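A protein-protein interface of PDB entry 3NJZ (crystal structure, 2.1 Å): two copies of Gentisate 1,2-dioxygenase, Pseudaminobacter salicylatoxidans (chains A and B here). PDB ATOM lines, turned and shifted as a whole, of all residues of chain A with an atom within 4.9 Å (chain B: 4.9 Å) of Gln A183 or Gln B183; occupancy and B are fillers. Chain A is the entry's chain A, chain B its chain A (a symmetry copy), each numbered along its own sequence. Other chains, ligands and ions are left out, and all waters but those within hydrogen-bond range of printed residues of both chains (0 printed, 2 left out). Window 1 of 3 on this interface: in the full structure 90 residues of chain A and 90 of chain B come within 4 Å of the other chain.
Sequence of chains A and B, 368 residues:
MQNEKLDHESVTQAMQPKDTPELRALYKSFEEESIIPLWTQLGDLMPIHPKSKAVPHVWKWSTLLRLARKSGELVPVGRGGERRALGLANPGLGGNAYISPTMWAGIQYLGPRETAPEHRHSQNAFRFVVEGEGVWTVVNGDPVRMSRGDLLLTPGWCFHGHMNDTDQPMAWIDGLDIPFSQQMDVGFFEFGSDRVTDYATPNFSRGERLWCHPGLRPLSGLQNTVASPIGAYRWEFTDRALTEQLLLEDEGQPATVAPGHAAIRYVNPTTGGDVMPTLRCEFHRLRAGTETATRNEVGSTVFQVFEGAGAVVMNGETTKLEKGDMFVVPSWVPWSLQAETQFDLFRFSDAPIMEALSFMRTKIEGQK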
ATOM      1  N   TYR A  98     -11.519 -26.542 -29.236  1.00  0.00           N
ATOM      2  CA  TYR A  98     -11.390 -27.173 -27.925  1.00  0.00           C
ATOM      3  C   TYR A  98     -12.488 -26.600 -27.048  1.00  0.00           C
ATOM      4  O   TYR A  98     -12.529 -25.381 -26.845  1.00  0.00           O
ATOM      5  CB  TYR A  98     -10.079 -26.766 -27.242  1.00  0.00           C
ATOM      6  CG  TYR A  98      -8.740 -27.099 -27.878  1.00  0.00           C
ATOM      7  CD1 TYR A  98      -8.629 -27.903 -29.013  1.00  0.00           C
ATOM      8  CD2 TYR A  98      -7.560 -26.617 -27.280  1.00  0.00           C
ATOM      9  CE1 TYR A  98      -7.367 -28.218 -29.546  1.00  0.00           C
ATOM     10  CE2 TYR A  98      -6.300 -26.924 -27.793  1.00  0.00           C
ATOM     11  CZ  TYR A  98      -6.207 -27.724 -28.921  1.00  0.00           C
ATOM     12  OH  TYR A  98      -4.953 -28.017 -29.399  1.00  0.00           O
ATOM     13  N   PRO A 101      -9.313 -27.198 -22.307  1.00  0.00           N
ATOM     14  CA  PRO A 101      -7.926 -27.548 -22.692  1.00  0.00           C
ATOM     15  C   PRO A 101      -7.677 -29.057 -22.921  1.00  0.00           C
ATOM     16  O   PRO A 101      -6.664 -29.443 -23.519  1.00  0.00           O
ATOM     17  CB  PRO A 101      -7.097 -27.084 -21.481  1.00  0.00           C
ATOM     18  CG  PRO A 101      -7.953 -25.958 -20.855  1.00  0.00           C
ATOM     19  CD  PRO A 101      -9.373 -26.471 -21.022  1.00  0.00           C
ATOM     20  N   ILE A 178      -9.263 -35.141 -27.790  1.00  0.00           N
ATOM     21  CA  ILE A 178      -8.525 -34.447 -28.873  1.00  0.00           C
ATOM     22  C   ILE A 178      -7.595 -33.293 -28.412  1.00  0.00           C
ATOM     23  O   ILE A 178      -6.432 -33.274 -28.786  1.00  0.00           O
ATOM     24  CB  ILE A 178      -9.499 -33.974 -30.000  1.00  0.00           C
ATOM     25  CG1 ILE A 178      -9.825 -35.136 -30.947  1.00  0.00           C
ATOM     26  CG2 ILE A 178      -8.941 -32.773 -30.810  1.00  0.00           C
ATOM     27  CD1 ILE A 178     -11.071 -34.869 -31.810  1.00  0.00           C
ATOM     28  N   PRO A 179      -8.104 -32.340 -27.586  1.00  0.00           N
ATOM     29  CA  PRO A 179      -7.227 -31.220 -27.222  1.00  0.00           C
ATOM     30  C   PRO A 179      -6.019 -31.669 -26.388  1.00  0.00           C
ATOM     31  O   PRO A 179      -4.893 -31.227 -26.662  1.00  0.00           O
ATOM     32  CB  PRO A 179      -8.145 -30.273 -26.435  1.00  0.00           C
ATOM     33  CG  PRO A 179      -9.527 -30.625 -26.949  1.00  0.00           C
ATOM     34  CD  PRO A 179      -9.480 -32.116 -27.114  1.00  0.00           C
ATOM     35  N   PHE A 180      -6.258 -32.546 -25.415  1.00  0.00           N
ATOM     36  CA  PHE A 180      -5.179 -33.118 -24.631  1.00  0.00           C
ATOM     37  C   PHE A 180      -4.185 -33.793 -25.549  1.00  0.00           C
ATOM     38  O   PHE A 180      -2.972 -33.587 -25.453  1.00  0.00           O
ATOM     39  CB  PHE A 180      -5.714 -34.150 -23.630  1.00  0.00           C
ATOM     40  CG  PHE A 180      -4.640 -34.754 -22.763  1.00  0.00           C
ATOM     41  CD1 PHE A 180      -4.010 -35.947 -23.128  1.00  0.00           C
ATOM     42  CD2 PHE A 180      -4.221 -34.098 -21.606  1.00  0.00           C
ATOM     43  CE1 PHE A 180      -2.974 -36.481 -22.341  1.00  0.00           C
ATOM     44  CE2 PHE A 180      -3.221 -34.646 -20.804  1.00  0.00           C
ATOM     45  CZ  PHE A 180      -2.596 -35.850 -21.188  1.00  0.00           C
ATOM     46  N   SER A 181      -4.706 -34.617 -26.442  1.00  0.00           N
ATOM     47  CA  SER A 181      -3.886 -35.419 -27.324  1.00  0.00           C
ATOM     48  C   SER A 181      -3.064 -34.593 -28.335  1.00  0.00           C
ATOM     49  O   SER A 181      -1.895 -34.912 -28.583  1.00  0.00           O
ATOM     50  CB  SER A 181      -4.768 -36.451 -28.034  1.00  0.00           C
ATOM     51  OG  SER A 181      -5.331 -37.409 -27.100  1.00  0.00           O
ATOM     52  N   GLN A 182      -3.665 -33.569 -28.935  1.00  0.00           N
ATOM     53  CA  GLN A 182      -2.912 -32.616 -29.750  1.00  0.00           C
ATOM     54  C   GLN A 182      -1.775 -31.908 -28.987  1.00  0.00           C
ATOM     55  O   GLN A 182      -0.621 -31.958 -29.418  1.00  0.00           O
ATOM     56  CB  GLN A 182      -3.822 -31.565 -30.394  1.00  0.00           C
ATOM     57  CG  GLN A 182      -3.032 -30.622 -31.323  1.00  0.00           C
ATOM     58  CD  GLN A 182      -3.936 -29.809 -32.187  1.00  0.00           C
ATOM     59  OE1 GLN A 182      -4.835 -29.095 -31.692  1.00  0.00           O
ATOM     60  NE2 GLN A 182      -3.732 -29.910 -33.499  1.00  0.00           N
ATOM     61  N   GLN A 183      -2.103 -31.249 -27.873  1.00  0.00           N
ATOM     62  CA  GLN A 183      -1.095 -30.484 -27.132  1.00  0.00           C
ATOM     63  C   GLN A 183       0.002 -31.367 -26.559  1.00  0.00           C
ATOM     64  O   GLN A 183       1.149 -30.926 -26.486  1.00  0.00           O
ATOM     65  CB  GLN A 183      -1.722 -29.666 -26.013  1.00  0.00           C
ATOM     66  CG  GLN A 183      -2.627 -28.532 -26.487  1.00  0.00           C
ATOM     67  CD  GLN A 183      -3.557 -28.045 -25.361  1.00  0.00           C
ATOM     68  OE1 GLN A 183      -4.469 -28.756 -24.946  1.00  0.00           O
ATOM     69  NE2 GLN A 183      -3.315 -26.855 -24.870  1.00  0.00           N
ATOM     70  N   MET A 184      -0.342 -32.605 -26.177  1.00  0.00           N
ATOM     71  CA  MET A 184       0.623 -33.524 -25.573  1.00  0.00           C
ATOM     72  C   MET A 184       1.374 -34.447 -26.540  1.00  0.00           C
ATOM     73  O   MET A 184       2.246 -35.194 -26.099  1.00  0.00           O
ATOM     74  CB  MET A 184      -0.060 -34.366 -24.485  1.00  0.00           C
ATOM     75  CG  MET A 184      -0.687 -33.506 -23.374  1.00  0.00           C
ATOM     76  SD  MET A 184       0.553 -32.394 -22.668  1.00  0.00           S
ATOM     77  CE  MET A 184       1.387 -33.719 -21.827  1.00  0.00           C
ATOM     78  N   ASP A 185       1.003 -34.425 -27.824  1.00  0.00           N
ATOM     79  CA  ASP A 185       1.675 -35.198 -28.909  1.00  0.00           C
ATOM     80  C   ASP A 185       1.559 -36.718 -28.763  1.00  0.00           C
ATOM     81  O   ASP A 185       2.563 -37.433 -28.864  1.00  0.00           O
ATOM     82  CB  ASP A 185       3.156 -34.801 -29.054  1.00  0.00           C
ATOM     83  CG  ASP A 185       3.356 -33.306 -29.311  1.00  0.00           C
ATOM     84  OD1 ASP A 185       2.537 -32.700 -30.054  1.00  0.00           O
ATOM     85  OD2 ASP A 185       4.351 -32.753 -28.773  1.00  0.00           O
ATOM     86  N   TYR B  98       8.918 -23.214 -22.435  1.00  0.00           N
ATOM     87  CA  TYR B  98       8.670 -24.652 -22.376  1.00  0.00           C
ATOM     88  C   TYR B  98       9.762 -25.325 -23.186  1.00  0.00           C
ATOM     89  O   TYR B  98       9.889 -25.044 -24.384  1.00  0.00           O
ATOM     90  CB  TYR B  98       7.360 -25.018 -23.086  1.00  0.00           C
ATOM     91  CG  TYR B  98       6.035 -24.455 -22.603  1.00  0.00           C
ATOM     92  CD1 TYR B  98       5.920 -23.714 -21.426  1.00  0.00           C
ATOM     93  CD2 TYR B  98       4.868 -24.724 -23.342  1.00  0.00           C
ATOM     94  CE1 TYR B  98       4.667 -23.245 -20.995  1.00  0.00           C
ATOM     95  CE2 TYR B  98       3.616 -24.271 -22.926  1.00  0.00           C
ATOM     96  CZ  TYR B  98       3.519 -23.536 -21.754  1.00  0.00           C
ATOM     97  OH  TYR B  98       2.273 -23.110 -21.365  1.00  0.00           O
ATOM     98  N   PRO B 101       6.302 -29.659 -24.660  1.00  0.00           N
ATOM     99  CA  PRO B 101       4.914 -29.329 -24.261  1.00  0.00           C
ATOM    100  C   PRO B 101       4.557 -29.682 -22.798  1.00  0.00           C
ATOM    101  O   PRO B 101       3.550 -29.201 -22.263  1.00  0.00           O
ATOM    102  CB  PRO B 101       4.062 -30.196 -25.205  1.00  0.00           C
ATOM    103  CG  PRO B 101       4.970 -30.404 -26.438  1.00  0.00           C
ATOM    104  CD  PRO B 101       6.352 -30.563 -25.827  1.00  0.00           C
ATOM    105  N   ILE B 178       5.908 -27.685 -15.219  1.00  0.00           N
ATOM    106  CA  ILE B 178       5.286 -26.363 -15.473  1.00  0.00           C
ATOM    107  C   ILE B 178       4.428 -26.267 -16.763  1.00  0.00           C
ATOM    108  O   ILE B 178       3.292 -25.823 -16.696  1.00  0.00           O
ATOM    109  CB  ILE B 178       6.353 -25.223 -15.415  1.00  0.00           C
ATOM    110  CG1 ILE B 178       6.635 -24.828 -13.960  1.00  0.00           C
ATOM    111  CG2 ILE B 178       5.936 -23.970 -16.232  1.00  0.00           C
ATOM    112  CD1 ILE B 178       7.942 -24.031 -13.802  1.00  0.00           C
ATOM    113  N   PRO B 179       4.967 -26.698 -17.935  1.00  0.00           N
ATOM    114  CA  PRO B 179       4.164 -26.529 -19.152  1.00  0.00           C
ATOM    115  C   PRO B 179       2.882 -27.373 -19.131  1.00  0.00           C
ATOM    116  O   PRO B 179       1.811 -26.861 -19.489  1.00  0.00           O
ATOM    117  CB  PRO B 179       5.112 -26.960 -20.281  1.00  0.00           C
ATOM    118  CG  PRO B 179       6.487 -26.735 -19.684  1.00  0.00           C
ATOM    119  CD  PRO B 179       6.329 -27.155 -18.252  1.00  0.00           C
ATOM    120  N   PHE B 180       2.998 -28.625 -18.692  1.00  0.00           N
ATOM    121  CA  PHE B 180       1.836 -29.480 -18.531  1.00  0.00           C
ATOM    122  C   PHE B 180       0.842 -28.817 -17.604  1.00  0.00           C
ATOM    123  O   PHE B 180      -0.354 -28.729 -17.895  1.00  0.00           O
ATOM    124  CB  PHE B 180       2.233 -30.841 -17.945  1.00  0.00           C
ATOM    125  CG  PHE B 180       1.070 -31.785 -17.787  1.00  0.00           C
ATOM    126  CD1 PHE B 180       0.367 -31.861 -16.581  1.00  0.00           C
ATOM    127  CD2 PHE B 180       0.644 -32.562 -18.864  1.00  0.00           C
ATOM    128  CE1 PHE B 180      -0.749 -32.707 -16.453  1.00  0.00           C
ATOM    129  CE2 PHE B 180      -0.437 -33.430 -18.727  1.00  0.00           C
ATOM    130  CZ  PHE B 180      -1.136 -33.493 -17.504  1.00  0.00           C
ATOM    131  N   SER B 181       1.342 -28.357 -16.470  1.00  0.00           N
ATOM    132  CA  SER B 181       0.509 -27.791 -15.432  1.00  0.00           C
ATOM    133  C   SER B 181      -0.190 -26.477 -15.839  1.00  0.00           C
ATOM    134  O   SER B 181      -1.366 -26.278 -15.511  1.00  0.00           O
ATOM    135  CB  SER B 181       1.341 -27.608 -14.160  1.00  0.00           C
ATOM    136  OG  SER B 181       1.776 -28.881 -13.614  1.00  0.00           O
ATOM    137  N   GLN B 182       0.522 -25.579 -16.513  1.00  0.00           N
ATOM    138  CA  GLN B 182      -0.108 -24.401 -17.110  1.00  0.00           C
ATOM    139  C   GLN B 182      -1.224 -24.737 -18.119  1.00  0.00           C
ATOM    140  O   GLN B 182      -2.354 -24.268 -17.966  1.00  0.00           O
ATOM    141  CB  GLN B 182       0.916 -23.476 -17.776  1.00  0.00           C
ATOM    142  CG  GLN B 182       0.254 -22.195 -18.321  1.00  0.00           C
ATOM    143  CD  GLN B 182       1.265 -21.159 -18.683  1.00  0.00           C
ATOM    144  OE1 GLN B 182       2.190 -21.410 -19.485  1.00  0.00           O
ATOM    145  NE2 GLN B 182       1.123 -19.976 -18.087  1.00  0.00           N
ATOM    146  N   GLN B 183      -0.903 -25.533 -19.143  1.00  0.00           N
ATOM    147  CA  GLN B 183      -1.885 -25.837 -20.189  1.00  0.00           C
ATOM    148  C   GLN B 183      -3.078 -26.618 -19.660  1.00  0.00           C
ATOM    149  O   GLN B 183      -4.188 -26.422 -20.155  1.00  0.00           O
ATOM    150  CB  GLN B 183      -1.255 -26.600 -21.345  1.00  0.00           C
ATOM    151  CG  GLN B 183      -0.238 -25.798 -22.154  1.00  0.00           C
ATOM    152  CD  GLN B 183       0.667 -26.719 -22.992  1.00  0.00           C
ATOM    153  OE1 GLN B 183       1.495 -27.448 -22.453  1.00  0.00           O
ATOM    154  NE2 GLN B 183       0.495 -26.691 -24.290  1.00  0.00           N
ATOM    155  N   MET B 184      -2.855 -27.474 -18.654  1.00  0.00           N
ATOM    156  CA  MET B 184      -3.921 -28.307 -18.097  1.00  0.00           C
ATOM    157  C   MET B 184      -4.691 -27.715 -16.911  1.00  0.00           C
ATOM    158  O   MET B 184      -5.642 -28.339 -16.443  1.00  0.00           O
ATOM    159  CB  MET B 184      -3.367 -29.687 -17.713  1.00  0.00           C
ATOM    160  CG  MET B 184      -2.733 -30.425 -18.904  1.00  0.00           C
ATOM    161  SD  MET B 184      -3.915 -30.546 -20.267  1.00  0.00           S
ATOM    162  CE  MET B 184      -4.896 -31.763 -19.423  1.00  0.00           C
ATOM    163  N   ASP B 185      -4.252 -26.557 -16.409  1.00  0.00           N
ATOM    164  CA  ASP B 185      -4.926 -25.804 -15.310  1.00  0.00           C
ATOM    165  C   ASP B 185      -4.939 -26.535 -13.964  1.00  0.00           C
ATOM    166  O   ASP B 185      -5.990 -26.638 -13.321  1.00  0.00           O
ATOM    167  CB  ASP B 185      -6.360 -25.399 -15.696  1.00  0.00           C
ATOM    168  CG  ASP B 185      -6.426 -24.569 -16.980  1.00  0.00           C
ATOM    169  OD1 ASP B 185      -5.523 -23.718 -17.203  1.00  0.00           O
ATOM    170  OD2 ASP B 185      -7.400 -24.771 -17.752  1.00  0.00           O
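OE1 of Gln A183 lies close to O of Pro A101. The side-chain amide oxygen (OE1) of Gln A183 sits close to the backbone carbonyl oxygen (O) of Pro A179, 3.0 Å away. OE1 of Gln B183 lies close to O of Pro B101, 2.7 Å away. The side-chain amide oxygen (OE1) of Gln B183 lies close to the backbone carbonyl oxygen (O) of Pro B179.
CB of Pro A101 touches O of Gln B183, 3.3 Å away. Pro A101 touches Asp B185. Phe A180 touches Phe B180. CE of Met B184 touches CD2 of Phe A180 (3.3 Å). Gln A183 touches Pro B101 (O to CB, 3.3 Å). Gln B183 touches Gln A183. CE of Met A184 touches CD2 of Phe B180 (3.3 Å). OD2 of Asp A185 touches CG of Pro B101 (3.4 Å).
Of the printed residues of chain B, Phe A180 touches Phe B180 (3.7 Å) and Met B184 (3.3 Å). Gln A183 touches two residues of chain B. Printed residues of chain B within 4 Å of Met A184: Phe B180. Of the printed residues of chain A, Pro B101 touches Gln A183 (3.3 Å) and Asp A185 (3.4 Å). Printed residues of chain A within 4 Å of Met B184: Phe A180 (3.3 Å). The nearest printed residue of chain B that does not touch Phe A180 is Gln B183 (7.8 Å).
Printed residues of chain A that touch a printed residue of chain B: Pro A101, Phe A180, Gln A183, Met A184 and Asp A185. Hydrophobic or aromatic side chains of chain A within 4 Å of the printed part of chain B: Pro A101, Phe A180 and Met A184. Along chain A the printed residues that touch a printed residue of chain B span positions 101 to 185. Of the 10 printed residues of chain B, 5 touch a printed residue of chain A. Hydrophobic or aromatic side chains of chain B within 4 Å of the printed part of chain A: Pro B101, Phe B180 and Met B184. Among the printed residues, 8 pairs touch across the chains. Among the printed residues, no Asp or Glu carboxylate lies within 4 Å of a Lys or Arg side-chain nitrogen of the other chain.
Pro A101 touches Gln B183, and with the chains exchanged Gln A183 touches Pro B101. Phe A180 touches its own counterpart, Phe B180. Phe A180 touches Met B184, and with the chains exchanged Met A184 touches Phe B180. Gln B183 touches its own counterpart, Gln A183.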
